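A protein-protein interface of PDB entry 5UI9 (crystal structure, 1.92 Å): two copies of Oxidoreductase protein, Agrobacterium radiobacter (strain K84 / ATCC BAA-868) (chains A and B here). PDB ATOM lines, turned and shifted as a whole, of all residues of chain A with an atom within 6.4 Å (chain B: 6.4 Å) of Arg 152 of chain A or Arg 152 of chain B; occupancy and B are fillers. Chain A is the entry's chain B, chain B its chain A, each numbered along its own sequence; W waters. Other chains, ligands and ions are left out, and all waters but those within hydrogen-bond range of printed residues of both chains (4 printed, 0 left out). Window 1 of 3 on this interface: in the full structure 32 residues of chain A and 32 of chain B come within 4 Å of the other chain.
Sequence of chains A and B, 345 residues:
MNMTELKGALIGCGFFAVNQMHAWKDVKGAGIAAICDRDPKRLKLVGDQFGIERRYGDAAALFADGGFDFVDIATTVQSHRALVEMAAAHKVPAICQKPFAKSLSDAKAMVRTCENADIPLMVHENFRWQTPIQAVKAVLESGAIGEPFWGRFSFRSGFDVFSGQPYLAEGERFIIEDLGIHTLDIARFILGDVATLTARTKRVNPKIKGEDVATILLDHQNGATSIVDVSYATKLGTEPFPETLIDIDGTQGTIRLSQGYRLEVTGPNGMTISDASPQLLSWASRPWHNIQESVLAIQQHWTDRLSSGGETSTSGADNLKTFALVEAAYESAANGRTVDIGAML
NH1 of Arg 152 of chain B lies within salt-bridge range of OD2 of Asp 247 of chain A, at 3.8 Å.
OD2 of Asp 247 of chain B lies within salt-bridge range of NH1 of Arg 152 of chain A, 3.4 Å away.
The guanidinium group (NH1) of Arg 152 of chain B sits close to the guanidinium group (NH1) of Arg 152 of chain A, at 3.2 Å.
The backbone NH (N) of Ile 227 of chain B lies within hydrogen-bond range of the backbone carbonyl oxygen (O) of Gly 151 of chain B.
OD2 of Asp 229 of chain B lies within hydrogen-bond range of OG of Ser 154 of chain B, at 2.6 Å.
NH1 of Arg 156 of chain B is in salt-bridge range of OD2 of Asp 229 of chain B (2.9 Å).
OG of Ser 154 of chain A is in hydrogen-bond range of NH2 of Arg 152 of chain A.
N of Phe 153 of chain A is in hydrogen-bond range of O of Ile 227 of chain A (2.9 Å).
The side-chain carboxylate of Asp 247 of chain A lies within salt-bridge range of the guanidinium group of Arg 256 of chain A, at 3.8 Å.
Among the printed residues, pairs that only touch across the chains: Trp 150 of chain A with Arg 152 of chain B (3.3 Å), Trp 150 of chain A with Arg 156 of chain B (3.3 Å), Trp 150 of chain A with Asp 229 of chain B (3.8 Å), Arg 152 of chain A with Trp 150 of chain B (3.3 Å), Arg 156 of chain A with Trp 150 of chain B (3.3 Å), Ile 227 of chain A with Ile 227 of chain B (3.6 Å) and Asp 229 of chain A with Trp 150 of chain B (3.8 Å).
Arg 152 of chain A touches just these residues of chain B: Trp 150 (3.3 Å), Arg 152 (3.2 Å) and Asp 247 (3.4 Å).
Arg 152 of chain B touches just these residues of chain A: Trp 150, Arg 152 and Asp 247.
Printed residues of chain A within 4 Å of Trp 150 of chain B: Arg 152 (3.3 Å), Arg 156 (3.3 Å) and Asp 229 (3.8 Å).
Of the printed residues of chain B, Trp 150 of chain A touches Arg 152, Arg 156 and Asp 229.
Thr 225 of chain A touches none of the printed residues of chain B.
The nearest residue of chain B that does not touch Arg 152 of chain A is Arg 256 of chain B (6.2 Å).
Printed residues of chain B that touch a printed residue of chain A: Trp 150, Arg 152, Arg 156, Ile 227, Asp 229 and Asp 247.
Among the printed residues, Asp or Glu carboxylates within 4 Å of a Lys or Arg side-chain nitrogen of the other chain: Arg 152 of chain A with Asp 247 of chain B and Asp 247 of chain A with Arg 152 of chain B.
Trp 150 of chain A touches Arg 152 of chain B, and with the chains exchanged Arg 152 of chain A touches Trp 150 of chain B.
Trp 150 of chain A touches Asp 229 of chain B, and with the chains exchanged Asp 229 of chain A touches Trp 150 of chain B.
Arg 152 of chain B touches its own counterpart, Arg 152 of chain A.
Arg 152 of chain A touches Asp 247 of chain B, and with the chains exchanged Asp 247 of chain A touches Arg 152 of chain B.
Positions printed for both chains: 150, 151, 152, 153, 154, 156, 191, 225, 226, 227, 228, 229, 245, 246, 247, 248 and 256.
Water W4 bridges OD2 of Asp 247 of chain A (2.7 Å) and NH2 of Arg 152 of chain B (2.8 Å).
Water W3 lies within hydrogen-bond range of the guanidinium group of Arg 156 of chain B (2.7 Å) and the indole nitrogen of Trp 150 of chain A (3.3 Å).
Water W2 lies within hydrogen-bond range of the side-chain carboxylate of Asp 247 of chain A, the guanidinium group of Arg 152 of chain A and the guanidinium group of Arg 152 of chain B.
Water W1 bridges NH1 of Arg 156 of chain A (2.8 Å) and NE1 of Trp 150 of chain B (3.4 Å).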
ATOM      1  N   TRP A 150       1.212   7.036 -13.334  1.00  0.00           N
ATOM      2  CA  TRP A 150       1.329   6.338 -12.070  1.00  0.00           C
ATOM      3  C   TRP A 150       1.460   4.838 -12.294  1.00  0.00           C
ATOM      4  O   TRP A 150       0.848   4.294 -13.204  1.00  0.00           O
ATOM      5  CB  TRP A 150       0.102   6.653 -11.194  1.00  0.00           C
ATOM      6  CG  TRP A 150       0.188   6.108  -9.821  1.00  0.00           C
ATOM      7  CD1 TRP A 150       0.749   6.706  -8.731  1.00  0.00           C
ATOM      8  CD2 TRP A 150      -0.298   4.841  -9.378  1.00  0.00           C
ATOM      9  NE1 TRP A 150       0.649   5.886  -7.639  1.00  0.00           N
ATOM     10  CE2 TRP A 150       0.004   4.736  -8.005  1.00  0.00           C
ATOM     11  CE3 TRP A 150      -0.967   3.788 -10.007  1.00  0.00           C
ATOM     12  CZ2 TRP A 150      -0.331   3.618  -7.255  1.00  0.00           C
ATOM     13  CZ3 TRP A 150      -1.305   2.677  -9.260  1.00  0.00           C
ATOM     14  CH2 TRP A 150      -0.990   2.603  -7.895  1.00  0.00           C
ATOM     15  N   GLY A 151       2.255   4.179 -11.457  1.00  0.00           N
ATOM     16  CA  GLY A 151       2.362   2.728 -11.480  1.00  0.00           C
ATOM     17  C   GLY A 151       2.513   2.099 -10.108  1.00  0.00           C
ATOM     18  O   GLY A 151       2.943   2.751  -9.159  1.00  0.00           O
ATOM     19  N   ARG A 152       2.121   0.833 -10.003  1.00  0.00           N
ATOM     20  CA  ARG A 152       2.485  -0.018  -8.882  1.00  0.00           C
ATOM     21  C   ARG A 152       3.057  -1.302  -9.443  1.00  0.00           C
ATOM     22  O   ARG A 152       2.461  -1.890 -10.349  1.00  0.00           O
ATOM     23  CB  ARG A 152       1.286  -0.369  -8.005  1.00  0.00           C
ATOM     24  CG  ARG A 152       1.676  -1.182  -6.774  1.00  0.00           C
ATOM     25  CD  ARG A 152       0.492  -1.862  -6.118  1.00  0.00           C
ATOM     26  NE  ARG A 152       0.912  -2.596  -4.923  1.00  0.00           N
ATOM     27  CZ  ARG A 152       0.125  -3.378  -4.184  1.00  0.00           C
ATOM     28  NH1 ARG A 152      -1.158  -3.542  -4.486  1.00  0.00           N
ATOM     29  NH2 ARG A 152       0.621  -3.995  -3.119  1.00  0.00           N
ATOM     30  N   PHE A 153       4.189  -1.731  -8.885  1.00  0.00           N
ATOM     31  CA  PHE A 153       4.845  -2.981  -9.252  1.00  0.00           C
ATOM     32  C   PHE A 153       5.053  -3.767  -7.966  1.00  0.00           C
ATOM     33  O   PHE A 153       5.854  -3.370  -7.122  1.00  0.00           O
ATOM     34  CB  PHE A 153       6.186  -2.709  -9.944  1.00  0.00           C
ATOM     35  CG  PHE A 153       6.083  -1.758 -11.095  1.00  0.00           C
ATOM     36  CD1 PHE A 153       6.164  -0.383 -10.887  1.00  0.00           C
ATOM     37  CD2 PHE A 153       5.881  -2.229 -12.390  1.00  0.00           C
ATOM     38  CE1 PHE A 153       6.044   0.500 -11.949  1.00  0.00           C
ATOM     39  CE2 PHE A 153       5.766  -1.353 -13.449  1.00  0.00           C
ATOM     40  CZ  PHE A 153       5.846   0.014 -13.232  1.00  0.00           C
ATOM     41  N   SER A 154       4.341  -4.884  -7.828  1.00  0.00           N
ATOM     42  CA  SER A 154       4.216  -5.575  -6.559  1.00  0.00           C
ATOM     43  C   SER A 154       4.580  -7.057  -6.674  1.00  0.00           C
ATOM     44  O   SER A 154       4.022  -7.769  -7.499  1.00  0.00           O
ATOM     45  CB  SER A 154       2.773  -5.428  -6.076  1.00  0.00           C
ATOM     46  OG  SER A 154       2.629  -5.884  -4.752  1.00  0.00           O
ATOM     47  N   ARG A 156       4.656  -9.830  -3.812  1.00  0.00           N
ATOM     48  CA  ARG A 156       4.410 -10.173  -2.412  1.00  0.00           C
ATOM     49  C   ARG A 156       4.137 -11.663  -2.336  1.00  0.00           C
ATOM     50  O   ARG A 156       3.138 -12.135  -2.871  1.00  0.00           O
ATOM     51  CB  ARG A 156       3.229  -9.380  -1.851  1.00  0.00           C
ATOM     52  CG  ARG A 156       3.317  -7.881  -2.105  1.00  0.00           C
ATOM     53  CD  ARG A 156       2.315  -7.114  -1.254  1.00  0.00           C
ATOM     54  NE  ARG A 156       2.770  -7.010   0.130  1.00  0.00           N
ATOM     55  CZ  ARG A 156       3.732  -6.194   0.571  1.00  0.00           C
ATOM     56  NH1 ARG A 156       4.380  -5.367  -0.258  1.00  0.00           N
ATOM     57  NH2 ARG A 156       4.058  -6.205   1.863  1.00  0.00           N
ATOM     58  N   LEU A 191       8.178   2.382 -17.105  1.00  0.00           N
ATOM     59  CA  LEU A 191       7.989   3.829 -16.911  1.00  0.00           C
ATOM     60  C   LEU A 191       9.242   4.706 -17.089  1.00  0.00           C
ATOM     61  O   LEU A 191       9.184   5.920 -16.866  1.00  0.00           O
ATOM     62  CB  LEU A 191       7.360   4.083 -15.532  1.00  0.00           C
ATOM     63  CG  LEU A 191       5.955   3.506 -15.327  1.00  0.00           C
ATOM     64  CD1 LEU A 191       5.488   3.753 -13.899  1.00  0.00           C
ATOM     65  CD2 LEU A 191       4.964   4.082 -16.326  1.00  0.00           C
ATOM     66  N   THR A 225       4.957   8.774 -11.175  1.00  0.00           N
ATOM     67  CA  THR A 225       5.262   8.331  -9.816  1.00  0.00           C
ATOM     68  C   THR A 225       4.939   6.850  -9.746  1.00  0.00           C
ATOM     69  O   THR A 225       3.934   6.428 -10.290  1.00  0.00           O
ATOM     70  CB  THR A 225       4.384   9.057  -8.784  1.00  0.00           C
ATOM     71  OG1 THR A 225       4.526  10.470  -8.935  1.00  0.00           O
ATOM     72  CG2 THR A 225       4.774   8.655  -7.354  1.00  0.00           C
ATOM     73  N   SER A 226       5.771   6.052  -9.092  1.00  0.00           N
ATOM     74  CA  SER A 226       5.427   4.638  -8.899  1.00  0.00           C
ATOM     75  C   SER A 226       5.810   4.085  -7.536  1.00  0.00           C
ATOM     76  O   SER A 226       6.686   4.617  -6.855  1.00  0.00           O
ATOM     77  CB  SER A 226       6.013   3.759 -10.014  1.00  0.00           C
ATOM     78  OG  SER A 226       7.392   3.519  -9.831  1.00  0.00           O
ATOM     79  N   ILE A 227       5.114   3.015  -7.161  1.00  0.00           N
ATOM     80  CA  ILE A 227       5.383   2.259  -5.953  1.00  0.00           C
ATOM     81  C   ILE A 227       5.973   0.920  -6.376  1.00  0.00           C
ATOM     82  O   ILE A 227       5.396   0.231  -7.206  1.00  0.00           O
ATOM     83  CB  ILE A 227       4.081   1.994  -5.171  1.00  0.00           C
ATOM     84  CG1 ILE A 227       3.415   3.310  -4.738  1.00  0.00           C
ATOM     85  CG2 ILE A 227       4.327   1.077  -3.975  1.00  0.00           C
ATOM     86  CD1 ILE A 227       4.238   4.148  -3.779  1.00  0.00           C
ATOM     87  N   VAL A 228       7.122   0.562  -5.817  1.00  0.00           N
ATOM     88  CA  VAL A 228       7.654  -0.789  -5.919  1.00  0.00           C
ATOM     89  C   VAL A 228       7.585  -1.363  -4.519  1.00  0.00           C
ATOM     90  O   VAL A 228       8.275  -0.873  -3.627  1.00  0.00           O
ATOM     91  CB  VAL A 228       9.103  -0.794  -6.446  1.00  0.00           C
ATOM     92  CG1 VAL A 228       9.775  -2.144  -6.226  1.00  0.00           C
ATOM     93  CG2 VAL A 228       9.114  -0.428  -7.924  1.00  0.00           C
ATOM     94  N   ASP A 229       6.755  -2.384  -4.325  1.00  0.00           N
ATOM     95  CA  ASP A 229       6.595  -2.997  -3.006  1.00  0.00           C
ATOM     96  C   ASP A 229       6.850  -4.491  -3.110  1.00  0.00           C
ATOM     97  O   ASP A 229       6.213  -5.181  -3.899  1.00  0.00           O
ATOM     98  CB  ASP A 229       5.226  -2.666  -2.382  1.00  0.00           C
ATOM     99  CG  ASP A 229       4.054  -3.236  -3.157  1.00  0.00           C
ATOM    100  OD1 ASP A 229       3.617  -2.605  -4.138  1.00  0.00           O
ATOM    101  OD2 ASP A 229       3.536  -4.304  -2.762  1.00  0.00           O
ATOM    102  N   LEU A 245       2.728  -8.268 -10.008  1.00  0.00           N
ATOM    103  CA  LEU A 245       1.443  -7.646 -10.324  1.00  0.00           C
ATOM    104  C   LEU A 245       1.663  -6.173 -10.617  1.00  0.00           C
ATOM    105  O   LEU A 245       2.430  -5.515  -9.923  1.00  0.00           O
ATOM    106  CB  LEU A 245       0.467  -7.814  -9.153  1.00  0.00           C
ATOM    107  CG  LEU A 245       0.380  -9.232  -8.582  1.00  0.00           C
ATOM    108  CD1 LEU A 245      -0.725  -9.282  -7.548  1.00  0.00           C
ATOM    109  CD2 LEU A 245       0.171 -10.267  -9.687  1.00  0.00           C
ATOM    110  N   ILE A 246       0.989  -5.659 -11.642  1.00  0.00           N
ATOM    111  CA  ILE A 246       1.292  -4.334 -12.160  1.00  0.00           C
ATOM    112  C   ILE A 246       0.022  -3.543 -12.404  1.00  0.00           C
ATOM    113  O   ILE A 246      -0.872  -4.006 -13.105  1.00  0.00           O
ATOM    114  CB  ILE A 246       2.118  -4.392 -13.467  1.00  0.00           C
ATOM    115  CG1 ILE A 246       3.436  -5.154 -13.237  1.00  0.00           C
ATOM    116  CG2 ILE A 246       2.376  -2.975 -13.991  1.00  0.00           C
ATOM    117  CD1 ILE A 246       4.249  -5.466 -14.474  1.00  0.00           C
ATOM    118  N   ASP A 247      -0.034  -2.342 -11.826  1.00  0.00           N
ATOM    119  CA  ASP A 247      -1.070  -1.362 -12.137  1.00  0.00           C
ATOM    120  C   ASP A 247      -0.407  -0.176 -12.810  1.00  0.00           C
ATOM    121  O   ASP A 247       0.571   0.326 -12.295  1.00  0.00           O
ATOM    122  CB  ASP A 247      -1.746  -0.871 -10.855  1.00  0.00           C
ATOM    123  CG  ASP A 247      -2.411  -1.983 -10.070  1.00  0.00           C
ATOM    124  OD1 ASP A 247      -2.429  -3.147 -10.524  1.00  0.00           O
ATOM    125  OD2 ASP A 247      -2.931  -1.676  -8.988  1.00  0.00           O
ATOM    126  N   ILE A 248      -0.924   0.260 -13.956  1.00  0.00           N
ATOM    127  CA  ILE A 248      -0.489   1.506 -14.581  1.00  0.00           C
ATOM    128  C   ILE A 248      -1.726   2.352 -14.821  1.00  0.00           C
ATOM    129  O   ILE A 248      -2.742   1.834 -15.291  1.00  0.00           O
ATOM    130  CB  ILE A 248       0.220   1.292 -15.948  1.00  0.00           C
ATOM    131  CG1 ILE A 248       1.334   0.240 -15.874  1.00  0.00           C
ATOM    132  CG2 ILE A 248       0.787   2.608 -16.475  1.00  0.00           C
ATOM    133  CD1 ILE A 248       2.554   0.649 -15.081  1.00  0.00           C
ATOM    134  N   ARG A 256      -4.118  -3.270 -15.745  1.00  0.00           N
ATOM    135  CA  ARG A 256      -4.168  -4.041 -14.502  1.00  0.00           C
ATOM    136  C   ARG A 256      -3.796  -5.495 -14.818  1.00  0.00           C
ATOM    137  O   ARG A 256      -4.601  -6.257 -15.386  1.00  0.00           O
ATOM    138  CB  ARG A 256      -5.556  -3.969 -13.852  1.00  0.00           C
ATOM    139  CG  ARG A 256      -5.988  -2.587 -13.359  1.00  0.00           C
ATOM    140  CD  ARG A 256      -5.246  -2.181 -12.097  1.00  0.00           C
ATOM    141  NE  ARG A 256      -5.684  -0.892 -11.550  1.00  0.00           N
ATOM    142  CZ  ARG A 256      -5.319   0.318 -11.998  1.00  0.00           C
ATOM    143  NH1 ARG A 256      -4.501   0.461 -13.045  1.00  0.00           N
ATOM    144  NH2 ARG A 256      -5.780   1.411 -11.386  1.00  0.00           N
ATOM    145  N   TRP B 150       2.509  -4.087   7.179  1.00  0.00           N
ATOM    146  CA  TRP B 150       2.445  -3.369   5.921  1.00  0.00           C
ATOM    147  C   TRP B 150       1.002  -3.185   5.508  1.00  0.00           C
ATOM    148  O   TRP B 150       0.176  -4.066   5.736  1.00  0.00           O
ATOM    149  CB  TRP B 150       3.202  -4.128   4.825  1.00  0.00           C
ATOM    150  CG  TRP B 150       3.326  -3.359   3.549  1.00  0.00           C
ATOM    151  CD1 TRP B 150       4.292  -2.448   3.227  1.00  0.00           C
ATOM    152  CD2 TRP B 150       2.442  -3.418   2.427  1.00  0.00           C
ATOM    153  NE1 TRP B 150       4.066  -1.939   1.973  1.00  0.00           N
ATOM    154  CE2 TRP B 150       2.940  -2.523   1.454  1.00  0.00           C
ATOM    155  CE3 TRP B 150       1.285  -4.153   2.140  1.00  0.00           C
ATOM    156  CZ2 TRP B 150       2.315  -2.336   0.223  1.00  0.00           C
ATOM    157  CZ3 TRP B 150       0.666  -3.969   0.906  1.00  0.00           C
ATOM    158  CH2 TRP B 150       1.185  -3.066  -0.032  1.00  0.00           C
ATOM    159  N   GLY B 151       0.703  -2.053   4.881  1.00  0.00           N
ATOM    160  CA  GLY B 151      -0.626  -1.841   4.320  1.00  0.00           C
ATOM    161  C   GLY B 151      -0.639  -1.003   3.063  1.00  0.00           C
ATOM    162  O   GLY B 151       0.291  -0.256   2.797  1.00  0.00           O
ATOM    163  N   ARG B 152      -1.704  -1.158   2.283  1.00  0.00           N
ATOM    164  CA  ARG B 152      -2.014  -0.254   1.202  1.00  0.00           C
ATOM    165  C   ARG B 152      -3.478   0.133   1.293  1.00  0.00           C
ATOM    166  O   ARG B 152      -4.337  -0.737   1.430  1.00  0.00           O
ATOM    167  CB  ARG B 152      -1.752  -0.902  -0.155  1.00  0.00           C
ATOM    168  CG  ARG B 152      -1.945   0.069  -1.316  1.00  0.00           C
ATOM    169  CD  ARG B 152      -2.301  -0.634  -2.608  1.00  0.00           C
ATOM    170  NE  ARG B 152      -2.442   0.322  -3.706  1.00  0.00           N
ATOM    171  CZ  ARG B 152      -2.879   0.021  -4.925  1.00  0.00           C
ATOM    172  NH1 ARG B 152      -3.223  -1.219  -5.246  1.00  0.00           N
ATOM    173  NH2 ARG B 152      -2.972   0.971  -5.837  1.00  0.00           N
ATOM    174  N   PHE B 153      -3.739   1.435   1.179  1.00  0.00           N
ATOM    175  CA  PHE B 153      -5.076   2.006   1.201  1.00  0.00           C
ATOM    176  C   PHE B 153      -5.222   2.839  -0.071  1.00  0.00           C
ATOM    177  O   PHE B 153      -4.515   3.827  -0.241  1.00  0.00           O
ATOM    178  CB  PHE B 153      -5.247   2.889   2.442  1.00  0.00           C
ATOM    179  CG  PHE B 153      -4.906   2.189   3.729  1.00  0.00           C
ATOM    180  CD1 PHE B 153      -3.585   2.143   4.186  1.00  0.00           C
ATOM    181  CD2 PHE B 153      -5.896   1.567   4.483  1.00  0.00           C
ATOM    182  CE1 PHE B 153      -3.264   1.485   5.364  1.00  0.00           C
ATOM    183  CE2 PHE B 153      -5.578   0.907   5.662  1.00  0.00           C
ATOM    184  CZ  PHE B 153      -4.261   0.865   6.102  1.00  0.00           C
ATOM    185  N   SER B 154      -6.145   2.448  -0.944  1.00  0.00           N
ATOM    186  CA  SER B 154      -6.190   2.948  -2.320  1.00  0.00           C
ATOM    187  C   SER B 154      -7.602   3.387  -2.709  1.00  0.00           C
ATOM    188  O   SER B 154      -8.557   2.642  -2.526  1.00  0.00           O
ATOM    189  CB  SER B 154      -5.705   1.850  -3.273  1.00  0.00           C
ATOM    190  OG  SER B 154      -5.612   2.323  -4.605  1.00  0.00           O
ATOM    191  N   ARG B 156      -8.870   4.966  -6.162  1.00  0.00           N
ATOM    192  CA  ARG B 156      -8.545   5.387  -7.527  1.00  0.00           C
ATOM    193  C   ARG B 156      -9.830   5.324  -8.335  1.00  0.00           C
ATOM    194  O   ARG B 156     -10.439   4.262  -8.450  1.00  0.00           O
ATOM    195  CB  ARG B 156      -7.470   4.492  -8.148  1.00  0.00           C
ATOM    196  CG  ARG B 156      -6.237   4.293  -7.275  1.00  0.00           C
ATOM    197  CD  ARG B 156      -5.076   3.697  -8.069  1.00  0.00           C
ATOM    198  NE  ARG B 156      -4.432   4.722  -8.902  1.00  0.00           N
ATOM    199  CZ  ARG B 156      -3.604   5.668  -8.456  1.00  0.00           C
ATOM    200  NH1 ARG B 156      -3.286   5.761  -7.163  1.00  0.00           N
ATOM    201  NH2 ARG B 156      -3.097   6.552  -9.314  1.00  0.00           N
ATOM    202  N   LEU B 191      -3.994   1.144  11.163  1.00  0.00           N
ATOM    203  CA  LEU B 191      -2.593   0.879  11.565  1.00  0.00           C
ATOM    204  C   LEU B 191      -2.012   1.854  12.594  1.00  0.00           C
ATOM    205  O   LEU B 191      -0.810   1.802  12.878  1.00  0.00           O
ATOM    206  CB  LEU B 191      -1.693   0.846  10.325  1.00  0.00           C
ATOM    207  CG  LEU B 191      -1.999  -0.235   9.290  1.00  0.00           C
ATOM    208  CD1 LEU B 191      -1.058  -0.087   8.106  1.00  0.00           C
ATOM    209  CD2 LEU B 191      -1.885  -1.628   9.890  1.00  0.00           C
ATOM    210  N   THR B 225       4.580   0.042   7.831  1.00  0.00           N
ATOM    211  CA  THR B 225       4.705   0.933   6.687  1.00  0.00           C
ATOM    212  C   THR B 225       3.416   0.837   5.894  1.00  0.00           C
ATOM    213  O   THR B 225       2.863  -0.250   5.753  1.00  0.00           O
ATOM    214  CB  THR B 225       5.860   0.497   5.771  1.00  0.00           C
ATOM    215  OG1 THR B 225       7.077   0.463   6.515  1.00  0.00           O
ATOM    216  CG2 THR B 225       6.016   1.447   4.582  1.00  0.00           C
ATOM    217  N   SER B 226       2.935   1.958   5.369  1.00  0.00           N
ATOM    218  CA  SER B 226       1.798   1.912   4.460  1.00  0.00           C
ATOM    219  C   SER B 226       1.911   2.883   3.287  1.00  0.00           C
ATOM    220  O   SER B 226       2.681   3.851   3.323  1.00  0.00           O
ATOM    221  CB  SER B 226       0.476   2.091   5.218  1.00  0.00           C
ATOM    222  OG  SER B 226       0.190   3.451   5.457  1.00  0.00           O
ATOM    223  N   ILE B 227       1.160   2.558   2.235  1.00  0.00           N
ATOM    224  CA  ILE B 227       0.961   3.410   1.075  1.00  0.00           C
ATOM    225  C   ILE B 227      -0.491   3.884   1.061  1.00  0.00           C
ATOM    226  O   ILE B 227      -1.415   3.075   1.171  1.00  0.00           O
ATOM    227  CB  ILE B 227       1.236   2.639  -0.236  1.00  0.00           C
ATOM    228  CG1 ILE B 227       2.704   2.190  -0.309  1.00  0.00           C
ATOM    229  CG2 ILE B 227       0.864   3.465  -1.465  1.00  0.00           C
ATOM    230  CD1 ILE B 227       3.717   3.320  -0.337  1.00  0.00           C
ATOM    231  N   VAL B 228      -0.678   5.193   0.934  1.00  0.00           N
ATOM    232  CA  VAL B 228      -1.977   5.781   0.637  1.00  0.00           C
ATOM    233  C   VAL B 228      -1.874   6.364  -0.762  1.00  0.00           C
ATOM    234  O   VAL B 228      -1.107   7.308  -0.996  1.00  0.00           O
ATOM    235  CB  VAL B 228      -2.362   6.869   1.648  1.00  0.00           C
ATOM    236  CG1 VAL B 228      -3.626   7.599   1.206  1.00  0.00           C
ATOM    237  CG2 VAL B 228      -2.559   6.240   3.014  1.00  0.00           C
ATOM    238  N   ASP B 229      -2.626   5.795  -1.694  1.00  0.00           N
ATOM    239  CA  ASP B 229      -2.610   6.270  -3.072  1.00  0.00           C
ATOM    240  C   ASP B 229      -4.026   6.630  -3.506  1.00  0.00           C
ATOM    241  O   ASP B 229      -4.942   5.819  -3.408  1.00  0.00           O
ATOM    242  CB  ASP B 229      -1.931   5.257  -4.005  1.00  0.00           C
ATOM    243  CG  ASP B 229      -2.672   3.940  -4.113  1.00  0.00           C
ATOM    244  OD1 ASP B 229      -2.447   3.046  -3.280  1.00  0.00           O
ATOM    245  OD2 ASP B 229      -3.448   3.773  -5.077  1.00  0.00           O
ATOM    246  N   LEU B 245      -9.871   0.365  -1.539  1.00  0.00           N
ATOM    247  CA  LEU B 245      -9.306  -0.982  -1.562  1.00  0.00           C
ATOM    248  C   LEU B 245      -8.163  -1.063  -0.555  1.00  0.00           C
ATOM    249  O   LEU B 245      -7.370  -0.133  -0.435  1.00  0.00           O
ATOM    250  CB  LEU B 245      -8.822  -1.340  -2.977  1.00  0.00           C
ATOM    251  CG  LEU B 245      -9.850  -1.063  -4.084  1.00  0.00           C
ATOM    252  CD1 LEU B 245      -9.344  -1.564  -5.431  1.00  0.00           C
ATOM    253  CD2 LEU B 245     -11.212  -1.674  -3.753  1.00  0.00           C
ATOM    254  N   ILE B 246      -8.085  -2.168   0.175  1.00  0.00           N
ATOM    255  CA  ILE B 246      -7.169  -2.272   1.307  1.00  0.00           C
ATOM    256  C   ILE B 246      -6.439  -3.611   1.321  1.00  0.00           C
ATOM    257  O   ILE B 246      -7.069  -4.672   1.264  1.00  0.00           O
ATOM    258  CB  ILE B 246      -7.896  -2.031   2.655  1.00  0.00           C
ATOM    259  CG1 ILE B 246      -8.479  -0.608   2.690  1.00  0.00           C
ATOM    260  CG2 ILE B 246      -6.932  -2.232   3.826  1.00  0.00           C
ATOM    261  CD1 ILE B 246      -9.303  -0.287   3.911  1.00  0.00           C
ATOM    262  N   ASP B 247      -5.108  -3.539   1.374  1.00  0.00           N
ATOM    263  CA  ASP B 247      -4.250  -4.699   1.602  1.00  0.00           C
ATOM    264  C   ASP B 247      -3.587  -4.500   2.953  1.00  0.00           C
ATOM    265  O   ASP B 247      -3.102  -3.410   3.229  1.00  0.00           O
ATOM    266  CB  ASP B 247      -3.151  -4.807   0.536  1.00  0.00           C
ATOM    267  CG  ASP B 247      -3.693  -4.893  -0.890  1.00  0.00           C
ATOM    268  OD1 ASP B 247      -4.921  -4.990  -1.096  1.00  0.00           O
ATOM    269  OD2 ASP B 247      -2.863  -4.853  -1.815  1.00  0.00           O
ATOM    270  N   ILE B 248      -3.586  -5.537   3.788  1.00  0.00           N
ATOM    271  CA  ILE B 248      -2.802  -5.554   5.020  1.00  0.00           C
ATOM    272  C   ILE B 248      -2.031  -6.863   5.091  1.00  0.00           C
ATOM    273  O   ILE B 248      -2.618  -7.928   4.892  1.00  0.00           O
ATOM    274  CB  ILE B 248      -3.687  -5.462   6.289  1.00  0.00           C
ATOM    275  CG1 ILE B 248      -4.704  -4.308   6.207  1.00  0.00           C
ATOM    276  CG2 ILE B 248      -2.819  -5.326   7.542  1.00  0.00           C
ATOM    277  CD1 ILE B 248      -4.103  -2.924   6.305  1.00  0.00           C
ATOM    278  N   ARG B 256      -7.254  -8.777   2.382  1.00  0.00           N
ATOM    279  CA  ARG B 256      -7.381  -8.179   1.053  1.00  0.00           C
ATOM    280  C   ARG B 256      -8.832  -7.779   0.810  1.00  0.00           C
ATOM    281  O   ARG B 256      -9.694  -8.631   0.562  1.00  0.00           O
ATOM    282  CB  ARG B 256      -6.899  -9.144  -0.036  1.00  0.00           C
ATOM    283  CG  ARG B 256      -5.403  -9.465   0.006  1.00  0.00           C
ATOM    284  CD  ARG B 256      -4.551  -8.323  -0.541  1.00  0.00           C
ATOM    285  NE  ARG B 256      -3.111  -8.620  -0.573  1.00  0.00           N
ATOM    286  CZ  ARG B 256      -2.279  -8.562   0.476  1.00  0.00           C
ATOM    287  NH1 ARG B 256      -2.713  -8.234   1.702  1.00  0.00           N
ATOM    288  NH2 ARG B 256      -0.991  -8.846   0.303  1.00  0.00           N
HETATM  289  O   HOH W   1       6.588  -4.019   0.904  1.00  0.00           O
HETATM  290  O   HOH W   2      -2.638  -3.773  -7.204  1.00  0.00           O
HETATM  291  O   HOH W   3      -1.746   7.971  -6.671  1.00  0.00           O
HETATM  292  O   HOH W   4      -4.689   0.106  -7.935  1.00  0.00           O
